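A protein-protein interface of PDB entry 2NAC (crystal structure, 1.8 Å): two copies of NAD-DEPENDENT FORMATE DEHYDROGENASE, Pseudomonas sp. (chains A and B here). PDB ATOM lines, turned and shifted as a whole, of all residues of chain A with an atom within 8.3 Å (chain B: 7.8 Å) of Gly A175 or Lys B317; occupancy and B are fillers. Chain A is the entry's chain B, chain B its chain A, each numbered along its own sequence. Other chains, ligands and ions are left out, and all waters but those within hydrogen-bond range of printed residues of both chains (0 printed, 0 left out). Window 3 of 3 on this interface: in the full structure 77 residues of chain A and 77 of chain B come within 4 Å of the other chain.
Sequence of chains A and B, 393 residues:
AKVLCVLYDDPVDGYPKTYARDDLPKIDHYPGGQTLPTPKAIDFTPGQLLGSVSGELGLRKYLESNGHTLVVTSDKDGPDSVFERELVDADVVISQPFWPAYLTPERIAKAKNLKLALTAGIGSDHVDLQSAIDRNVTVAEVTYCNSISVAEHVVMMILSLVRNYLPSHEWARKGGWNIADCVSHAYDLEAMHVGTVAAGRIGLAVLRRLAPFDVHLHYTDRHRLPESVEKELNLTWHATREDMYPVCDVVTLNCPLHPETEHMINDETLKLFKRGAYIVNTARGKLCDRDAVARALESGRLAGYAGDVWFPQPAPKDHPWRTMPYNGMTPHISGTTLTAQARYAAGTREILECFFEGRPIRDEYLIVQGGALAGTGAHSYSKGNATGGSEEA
The guanidinium group (NH1) of Arg B322 sits at hydrogen-bond distance from the backbone carbonyl oxygen (O) of Gly A176, 2.9 Å away. The guanidinium group (NH1) of Arg B322 lies within hydrogen-bond range of the backbone carbonyl oxygen (O) of Ala A172, 2.8 Å away.
The backbone carbonyl oxygen (O) of Ala B315 sits at hydrogen-bond distance from the guanidinium group (NH2) of Arg B322 (2.8 Å). OE1 of Glu A170 is in salt-bridge range of NH2 of Arg A173, 2.5 Å away. The backbone NH (N) of Gly A176 is in hydrogen-bond range of the backbone carbonyl oxygen (O) of Trp A171 (2.9 Å). The backbone carbonyl oxygen of Lys B317 sits close to the guanidinium group of Arg B322 (3.4 Å). The guanidinium group of Arg B322 lies within hydrogen-bond range of the backbone carbonyl oxygen of Pro B316 (2.9 Å).
Among the printed residues, pairs that only touch across the chains: Trp A171 with Arg B322, Arg A173 with Arg B322, Gly A175 with Lys B317, Gly A175 with Arg B322, Trp A177 with Trp B310, Trp A177 with Pro B314 and Trp A177 with Ala B315.
Of the printed residues of chain B, Trp A171 touches Arg B322 (3.9 Å). Of chain B, only Lys B317 and Arg B322 come within 4 Å of Gly A175. Printed residues of chain B within 4 Å of Gly A176: Arg B322. Printed residues of chain B within 4 Å of Trp A177: Trp B310, Pro B314 and Ala B315. Of the printed residues of chain A, Trp B310 touches Trp A177 (3.3 Å). Printed residues of chain A within 4 Å of Pro B314: Trp A177 (3.7 Å). Printed residues of chain A within 4 Å of Ala B315: Trp A177 (3.6 Å). Of chain A, only Gly A175 (3.97 Å) comes within 4 Å of Lys B317.
Of the 10 printed residues of chain B, 5 touch a printed residue of chain A. Printed residues of chain B that touch a printed residue of chain A: Trp B310, Pro B314, Ala B315, Lys B317 and Arg B322. Hydrophobic or aromatic side chains of chain B within 4 Å of the printed part of chain A: Trp B310, Pro B314 and Ala B315. Printed residues of chain A that touch a printed residue of chain B: Trp A171, Ala A172, Arg A173, Gly A175, Gly A176 and Trp A177. Hydrophobic or aromatic side chains of chain A that line the printed part of chain B: Trp A177. Among the printed residues, 9 pairs touch across the chains. Among the printed residues, no Asp or Glu carboxylate lies within 4 Å of a Lys or Arg side-chain nitrogen of the other chain.
No position is printed for both chains. Of the 9 pairs that touch across the chains among the printed residues, none has its exchanged pair printed and touching as well.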
ATOM      1  N   HIS A 169      18.860  -6.217 -17.093  1.00  0.00           N
ATOM      2  CA  HIS A 169      19.431  -4.911 -17.375  1.00  0.00           C
ATOM      3  C   HIS A 169      20.958  -4.970 -17.429  1.00  0.00           C
ATOM      4  O   HIS A 169      21.618  -4.375 -18.302  1.00  0.00           O
ATOM      5  CB  HIS A 169      18.937  -3.846 -16.406  1.00  0.00           C
ATOM      6  CG  HIS A 169      19.574  -2.523 -16.719  1.00  0.00           C
ATOM      7  ND1 HIS A 169      19.320  -1.815 -17.892  1.00  0.00           N
ATOM      8  CD2 HIS A 169      20.485  -1.802 -15.989  1.00  0.00           C
ATOM      9  CE1 HIS A 169      20.023  -0.710 -17.872  1.00  0.00           C
ATOM     10  NE2 HIS A 169      20.734  -0.663 -16.740  1.00  0.00           N
ATOM     11  N   GLU A 170      21.582  -5.720 -16.580  1.00  0.00           N
ATOM     12  CA  GLU A 170      23.038  -5.895 -16.559  1.00  0.00           C
ATOM     13  C   GLU A 170      23.542  -6.504 -17.868  1.00  0.00           C
ATOM     14  O   GLU A 170      24.538  -6.019 -18.454  1.00  0.00           O
ATOM     15  CB  GLU A 170      23.510  -6.784 -15.416  1.00  0.00           C
ATOM     16  CG  GLU A 170      23.661  -6.122 -14.078  1.00  0.00           C
ATOM     17  CD  GLU A 170      24.650  -4.956 -14.046  1.00  0.00           C
ATOM     18  OE1 GLU A 170      25.843  -5.355 -13.956  1.00  0.00           O
ATOM     19  OE2 GLU A 170      24.208  -3.764 -14.092  1.00  0.00           O
ATOM     20  N   TRP A 171      22.845  -7.542 -18.342  1.00  0.00           N
ATOM     21  CA  TRP A 171      23.206  -8.156 -19.625  1.00  0.00           C
ATOM     22  C   TRP A 171      23.134  -7.114 -20.720  1.00  0.00           C
ATOM     23  O   TRP A 171      24.010  -7.091 -21.555  1.00  0.00           O
ATOM     24  CB  TRP A 171      22.279  -9.271 -20.015  1.00  0.00           C
ATOM     25  CG  TRP A 171      22.583 -10.529 -19.305  1.00  0.00           C
ATOM     26  CD1 TRP A 171      21.822 -11.077 -18.329  1.00  0.00           C
ATOM     27  CD2 TRP A 171      23.669 -11.421 -19.480  1.00  0.00           C
ATOM     28  NE1 TRP A 171      22.395 -12.241 -17.878  1.00  0.00           N
ATOM     29  CE2 TRP A 171      23.508 -12.480 -18.596  1.00  0.00           C
ATOM     30  CE3 TRP A 171      24.761 -11.417 -20.354  1.00  0.00           C
ATOM     31  CZ2 TRP A 171      24.414 -13.538 -18.543  1.00  0.00           C
ATOM     32  CZ3 TRP A 171      25.653 -12.455 -20.315  1.00  0.00           C
ATOM     33  CH2 TRP A 171      25.468 -13.517 -19.404  1.00  0.00           C
ATOM     34  N   ALA A 172      22.129  -6.251 -20.762  1.00  0.00           N
ATOM     35  CA  ALA A 172      22.031  -5.210 -21.773  1.00  0.00           C
ATOM     36  C   ALA A 172      23.192  -4.187 -21.682  1.00  0.00           C
ATOM     37  O   ALA A 172      23.896  -3.812 -22.622  1.00  0.00           O
ATOM     38  CB  ALA A 172      20.720  -4.491 -21.670  1.00  0.00           C
ATOM     39  N   ARG A 173      23.403  -3.712 -20.451  1.00  0.00           N
ATOM     40  CA  ARG A 173      24.424  -2.711 -20.168  1.00  0.00           C
ATOM     41  C   ARG A 173      25.808  -3.251 -20.471  1.00  0.00           C
ATOM     42  O   ARG A 173      26.619  -2.433 -20.971  1.00  0.00           O
ATOM     43  CB  ARG A 173      24.367  -2.433 -18.667  1.00  0.00           C
ATOM     44  CG  ARG A 173      24.750  -1.140 -18.108  1.00  0.00           C
ATOM     45  CD  ARG A 173      24.436  -1.140 -16.600  1.00  0.00           C
ATOM     46  NE  ARG A 173      25.193  -1.991 -15.718  1.00  0.00           N
ATOM     47  CZ  ARG A 173      26.474  -2.246 -15.516  1.00  0.00           C
ATOM     48  NH1 ARG A 173      27.549  -1.755 -16.137  1.00  0.00           N
ATOM     49  NH2 ARG A 173      26.871  -3.115 -14.581  1.00  0.00           N
ATOM     50  N   LYS A 174      26.099  -4.505 -20.243  1.00  0.00           N
ATOM     51  CA  LYS A 174      27.411  -5.017 -20.496  1.00  0.00           C
ATOM     52  C   LYS A 174      27.703  -5.561 -21.867  1.00  0.00           C
ATOM     53  O   LYS A 174      28.783  -6.134 -22.048  1.00  0.00           O
ATOM     54  CB  LYS A 174      27.693  -6.084 -19.431  1.00  0.00           C
ATOM     55  CG  LYS A 174      27.443  -5.509 -18.046  1.00  0.00           C
ATOM     56  CD  LYS A 174      28.583  -5.308 -17.109  1.00  0.00           C
ATOM     57  CE  LYS A 174      28.730  -6.548 -16.212  1.00  0.00           C
ATOM     58  NZ  LYS A 174      29.611  -6.237 -15.034  1.00  0.00           N
ATOM     59  N   GLY A 175      26.864  -5.416 -22.871  1.00  0.00           N
ATOM     60  CA  GLY A 175      27.131  -5.888 -24.206  1.00  0.00           C
ATOM     61  C   GLY A 175      26.560  -7.241 -24.561  1.00  0.00           C
ATOM     62  O   GLY A 175      26.854  -7.657 -25.680  1.00  0.00           O
ATOM     63  N   GLY A 176      25.806  -7.851 -23.669  1.00  0.00           N
ATOM     64  CA  GLY A 176      25.180  -9.138 -23.887  1.00  0.00           C
ATOM     65  C   GLY A 176      23.839  -9.058 -24.603  1.00  0.00           C
ATOM     66  O   GLY A 176      23.326  -8.050 -25.059  1.00  0.00           O
ATOM     67  N   TRP A 177      23.186 -10.188 -24.746  1.00  0.00           N
ATOM     68  CA  TRP A 177      21.889 -10.446 -25.375  1.00  0.00           C
ATOM     69  C   TRP A 177      21.306 -11.532 -24.468  1.00  0.00           C
ATOM     70  O   TRP A 177      20.499 -11.230 -23.591  1.00  0.00           O
ATOM     71  CB  TRP A 177      21.969 -10.732 -26.852  1.00  0.00           C
ATOM     72  CG  TRP A 177      20.603 -10.540 -27.448  1.00  0.00           C
ATOM     73  CD1 TRP A 177      19.819 -11.555 -27.978  1.00  0.00           C
ATOM     74  CD2 TRP A 177      19.922  -9.298 -27.637  1.00  0.00           C
ATOM     75  NE1 TRP A 177      18.673 -10.987 -28.435  1.00  0.00           N
ATOM     76  CE2 TRP A 177      18.683  -9.631 -28.254  1.00  0.00           C
ATOM     77  CE3 TRP A 177      20.198  -7.958 -27.291  1.00  0.00           C
ATOM     78  CZ2 TRP A 177      17.738  -8.647 -28.538  1.00  0.00           C
ATOM     79  CZ3 TRP A 177      19.241  -7.031 -27.584  1.00  0.00           C
ATOM     80  CH2 TRP A 177      18.039  -7.381 -28.226  1.00  0.00           C
ATOM     81  N   ASN A 178      21.789 -12.760 -24.642  1.00  0.00           N
ATOM     82  CA  ASN A 178      21.497 -13.797 -23.702  1.00  0.00           C
ATOM     83  C   ASN A 178      20.135 -13.903 -23.100  1.00  0.00           C
ATOM     84  O   ASN A 178      19.872 -13.904 -21.890  1.00  0.00           O
ATOM     85  CB  ASN A 178      22.447 -13.401 -22.490  1.00  0.00           C
ATOM     86  CG  ASN A 178      23.900 -13.485 -22.924  1.00  0.00           C
ATOM     87  OD1 ASN A 178      24.493 -12.578 -23.495  1.00  0.00           O
ATOM     88  ND2 ASN A 178      24.527 -14.629 -22.758  1.00  0.00           N
ATOM     89  N   TRP B 310      14.888  -3.365 -29.848  1.00  0.00           N
ATOM     90  CA  TRP B 310      15.982  -2.716 -30.467  1.00  0.00           C
ATOM     91  C   TRP B 310      16.062  -2.893 -32.012  1.00  0.00           C
ATOM     92  O   TRP B 310      15.452  -3.776 -32.548  1.00  0.00           O
ATOM     93  CB  TRP B 310      17.321  -3.287 -29.928  1.00  0.00           C
ATOM     94  CG  TRP B 310      17.424  -3.582 -28.443  1.00  0.00           C
ATOM     95  CD1 TRP B 310      16.682  -4.398 -27.639  1.00  0.00           C
ATOM     96  CD2 TRP B 310      18.423  -3.010 -27.570  1.00  0.00           C
ATOM     97  NE1 TRP B 310      17.114  -4.361 -26.319  1.00  0.00           N
ATOM     98  CE2 TRP B 310      18.227  -3.568 -26.282  1.00  0.00           C
ATOM     99  CE3 TRP B 310      19.491  -2.142 -27.771  1.00  0.00           C
ATOM    100  CZ2 TRP B 310      19.051  -3.254 -25.199  1.00  0.00           C
ATOM    101  CZ3 TRP B 310      20.275  -1.812 -26.657  1.00  0.00           C
ATOM    102  CH2 TRP B 310      20.033  -2.350 -25.390  1.00  0.00           C
ATOM    103  N   PRO B 314      19.923  -9.172 -32.817  1.00  0.00           N
ATOM    104  CA  PRO B 314      20.403  -8.739 -31.505  1.00  0.00           C
ATOM    105  C   PRO B 314      21.129  -7.438 -31.677  1.00  0.00           C
ATOM    106  O   PRO B 314      21.692  -7.083 -32.727  1.00  0.00           O
ATOM    107  CB  PRO B 314      21.310  -9.871 -30.967  1.00  0.00           C
ATOM    108  CG  PRO B 314      21.640 -10.646 -32.211  1.00  0.00           C
ATOM    109  CD  PRO B 314      20.633 -10.381 -33.277  1.00  0.00           C
ATOM    110  N   ALA B 315      21.091  -6.601 -30.630  1.00  0.00           N
ATOM    111  CA  ALA B 315      21.739  -5.298 -30.698  1.00  0.00           C
ATOM    112  C   ALA B 315      23.230  -5.511 -30.685  1.00  0.00           C
ATOM    113  O   ALA B 315      23.774  -6.282 -29.904  1.00  0.00           O
ATOM    114  CB  ALA B 315      21.312  -4.528 -29.442  1.00  0.00           C
ATOM    115  N   PRO B 316      23.953  -4.814 -31.543  1.00  0.00           N
ATOM    116  CA  PRO B 316      25.389  -4.820 -31.610  1.00  0.00           C
ATOM    117  C   PRO B 316      25.882  -4.409 -30.211  1.00  0.00           C
ATOM    118  O   PRO B 316      25.250  -3.691 -29.424  1.00  0.00           O
ATOM    119  CB  PRO B 316      25.853  -3.824 -32.667  1.00  0.00           C
ATOM    120  CG  PRO B 316      24.576  -3.286 -33.202  1.00  0.00           C
ATOM    121  CD  PRO B 316      23.375  -3.875 -32.515  1.00  0.00           C
ATOM    122  N   LYS B 317      27.047  -4.885 -29.875  1.00  0.00           N
ATOM    123  CA  LYS B 317      27.649  -4.648 -28.555  1.00  0.00           C
ATOM    124  C   LYS B 317      27.857  -3.183 -28.278  1.00  0.00           C
ATOM    125  O   LYS B 317      27.818  -2.774 -27.128  1.00  0.00           O
ATOM    126  CB  LYS B 317      28.909  -5.503 -28.491  1.00  0.00           C
ATOM    127  CG  LYS B 317      29.752  -5.434 -27.248  1.00  0.00           C
ATOM    128  CD  LYS B 317      30.945  -6.376 -27.302  1.00  0.00           C
ATOM    129  CE  LYS B 317      30.688  -7.816 -26.848  1.00  0.00           C
ATOM    130  NZ  LYS B 317      31.960  -8.626 -26.774  1.00  0.00           N
ATOM    131  N   ASP B 318      28.064  -2.344 -29.250  1.00  0.00           N
ATOM    132  CA  ASP B 318      28.256  -0.923 -29.154  1.00  0.00           C
ATOM    133  C   ASP B 318      26.976  -0.137 -29.406  1.00  0.00           C
ATOM    134  O   ASP B 318      27.026   1.090 -29.623  1.00  0.00           O
ATOM    135  CB  ASP B 318      29.358  -0.495 -30.151  1.00  0.00           C
ATOM    136  CG  ASP B 318      29.065  -0.636 -31.627  1.00  0.00           C
ATOM    137  OD1 ASP B 318      28.050  -1.147 -32.162  1.00  0.00           O
ATOM    138  OD2 ASP B 318      29.905  -0.194 -32.473  1.00  0.00           O
ATOM    139  N   HIS B 319      25.806  -0.778 -29.387  1.00  0.00           N
ATOM    140  CA  HIS B 319      24.586   0.004 -29.650  1.00  0.00           C
ATOM    141  C   HIS B 319      24.484   1.062 -28.557  1.00  0.00           C
ATOM    142  O   HIS B 319      24.606   0.726 -27.384  1.00  0.00           O
ATOM    143  CB  HIS B 319      23.447  -0.998 -29.590  1.00  0.00           C
ATOM    144  CG  HIS B 319      22.166  -0.387 -29.976  1.00  0.00           C
ATOM    145  ND1 HIS B 319      21.495   0.621 -29.390  1.00  0.00           N
ATOM    146  CD2 HIS B 319      21.389  -0.748 -31.051  1.00  0.00           C
ATOM    147  CE1 HIS B 319      20.370   0.896 -30.030  1.00  0.00           C
ATOM    148  NE2 HIS B 319      20.290   0.022 -31.039  1.00  0.00           N
ATOM    149  N   PRO B 320      24.246   2.308 -28.904  1.00  0.00           N
ATOM    150  CA  PRO B 320      24.166   3.444 -28.006  1.00  0.00           C
ATOM    151  C   PRO B 320      23.139   3.366 -26.901  1.00  0.00           C
ATOM    152  O   PRO B 320      23.371   3.970 -25.814  1.00  0.00           O
ATOM    153  CB  PRO B 320      23.931   4.660 -28.910  1.00  0.00           C
ATOM    154  CG  PRO B 320      23.308   4.044 -30.131  1.00  0.00           C
ATOM    155  CD  PRO B 320      24.046   2.736 -30.301  1.00  0.00           C
ATOM    156  N   ARG B 322      22.524   0.929 -24.961  1.00  0.00           N
ATOM    157  CA  ARG B 322      23.040   0.112 -23.916  1.00  0.00           C
ATOM    158  C   ARG B 322      23.602   0.981 -22.771  1.00  0.00           C
ATOM    159  O   ARG B 322      23.502   0.637 -21.601  1.00  0.00           O
ATOM    160  CB  ARG B 322      24.127  -0.872 -24.337  1.00  0.00           C
ATOM    161  CG  ARG B 322      23.727  -1.921 -25.364  1.00  0.00           C
ATOM    162  CD  ARG B 322      24.921  -2.749 -25.718  1.00  0.00           C
ATOM    163  NE  ARG B 322      24.590  -3.835 -26.635  1.00  0.00           N
ATOM    164  CZ  ARG B 322      24.109  -4.977 -26.275  1.00  0.00           C
ATOM    165  NH1 ARG B 322      23.885  -5.238 -24.983  1.00  0.00           N
ATOM    166  NH2 ARG B 322      23.852  -5.978 -27.099  1.00  0.00           N
ATOM    167  N   THR B 323      24.198   2.055 -23.224  1.00  0.00           N
ATOM    168  CA  THR B 323      24.891   2.940 -22.300  1.00  0.00           C
ATOM    169  C   THR B 323      24.442   4.372 -22.231  1.00  0.00           C
ATOM    170  O   THR B 323      25.026   5.084 -21.417  1.00  0.00           O
ATOM    171  CB  THR B 323      26.426   2.932 -22.601  1.00  0.00           C
ATOM    172  OG1 THR B 323      26.620   3.402 -23.926  1.00  0.00           O
ATOM    173  CG2 THR B 323      27.033   1.553 -22.430  1.00  0.00           C
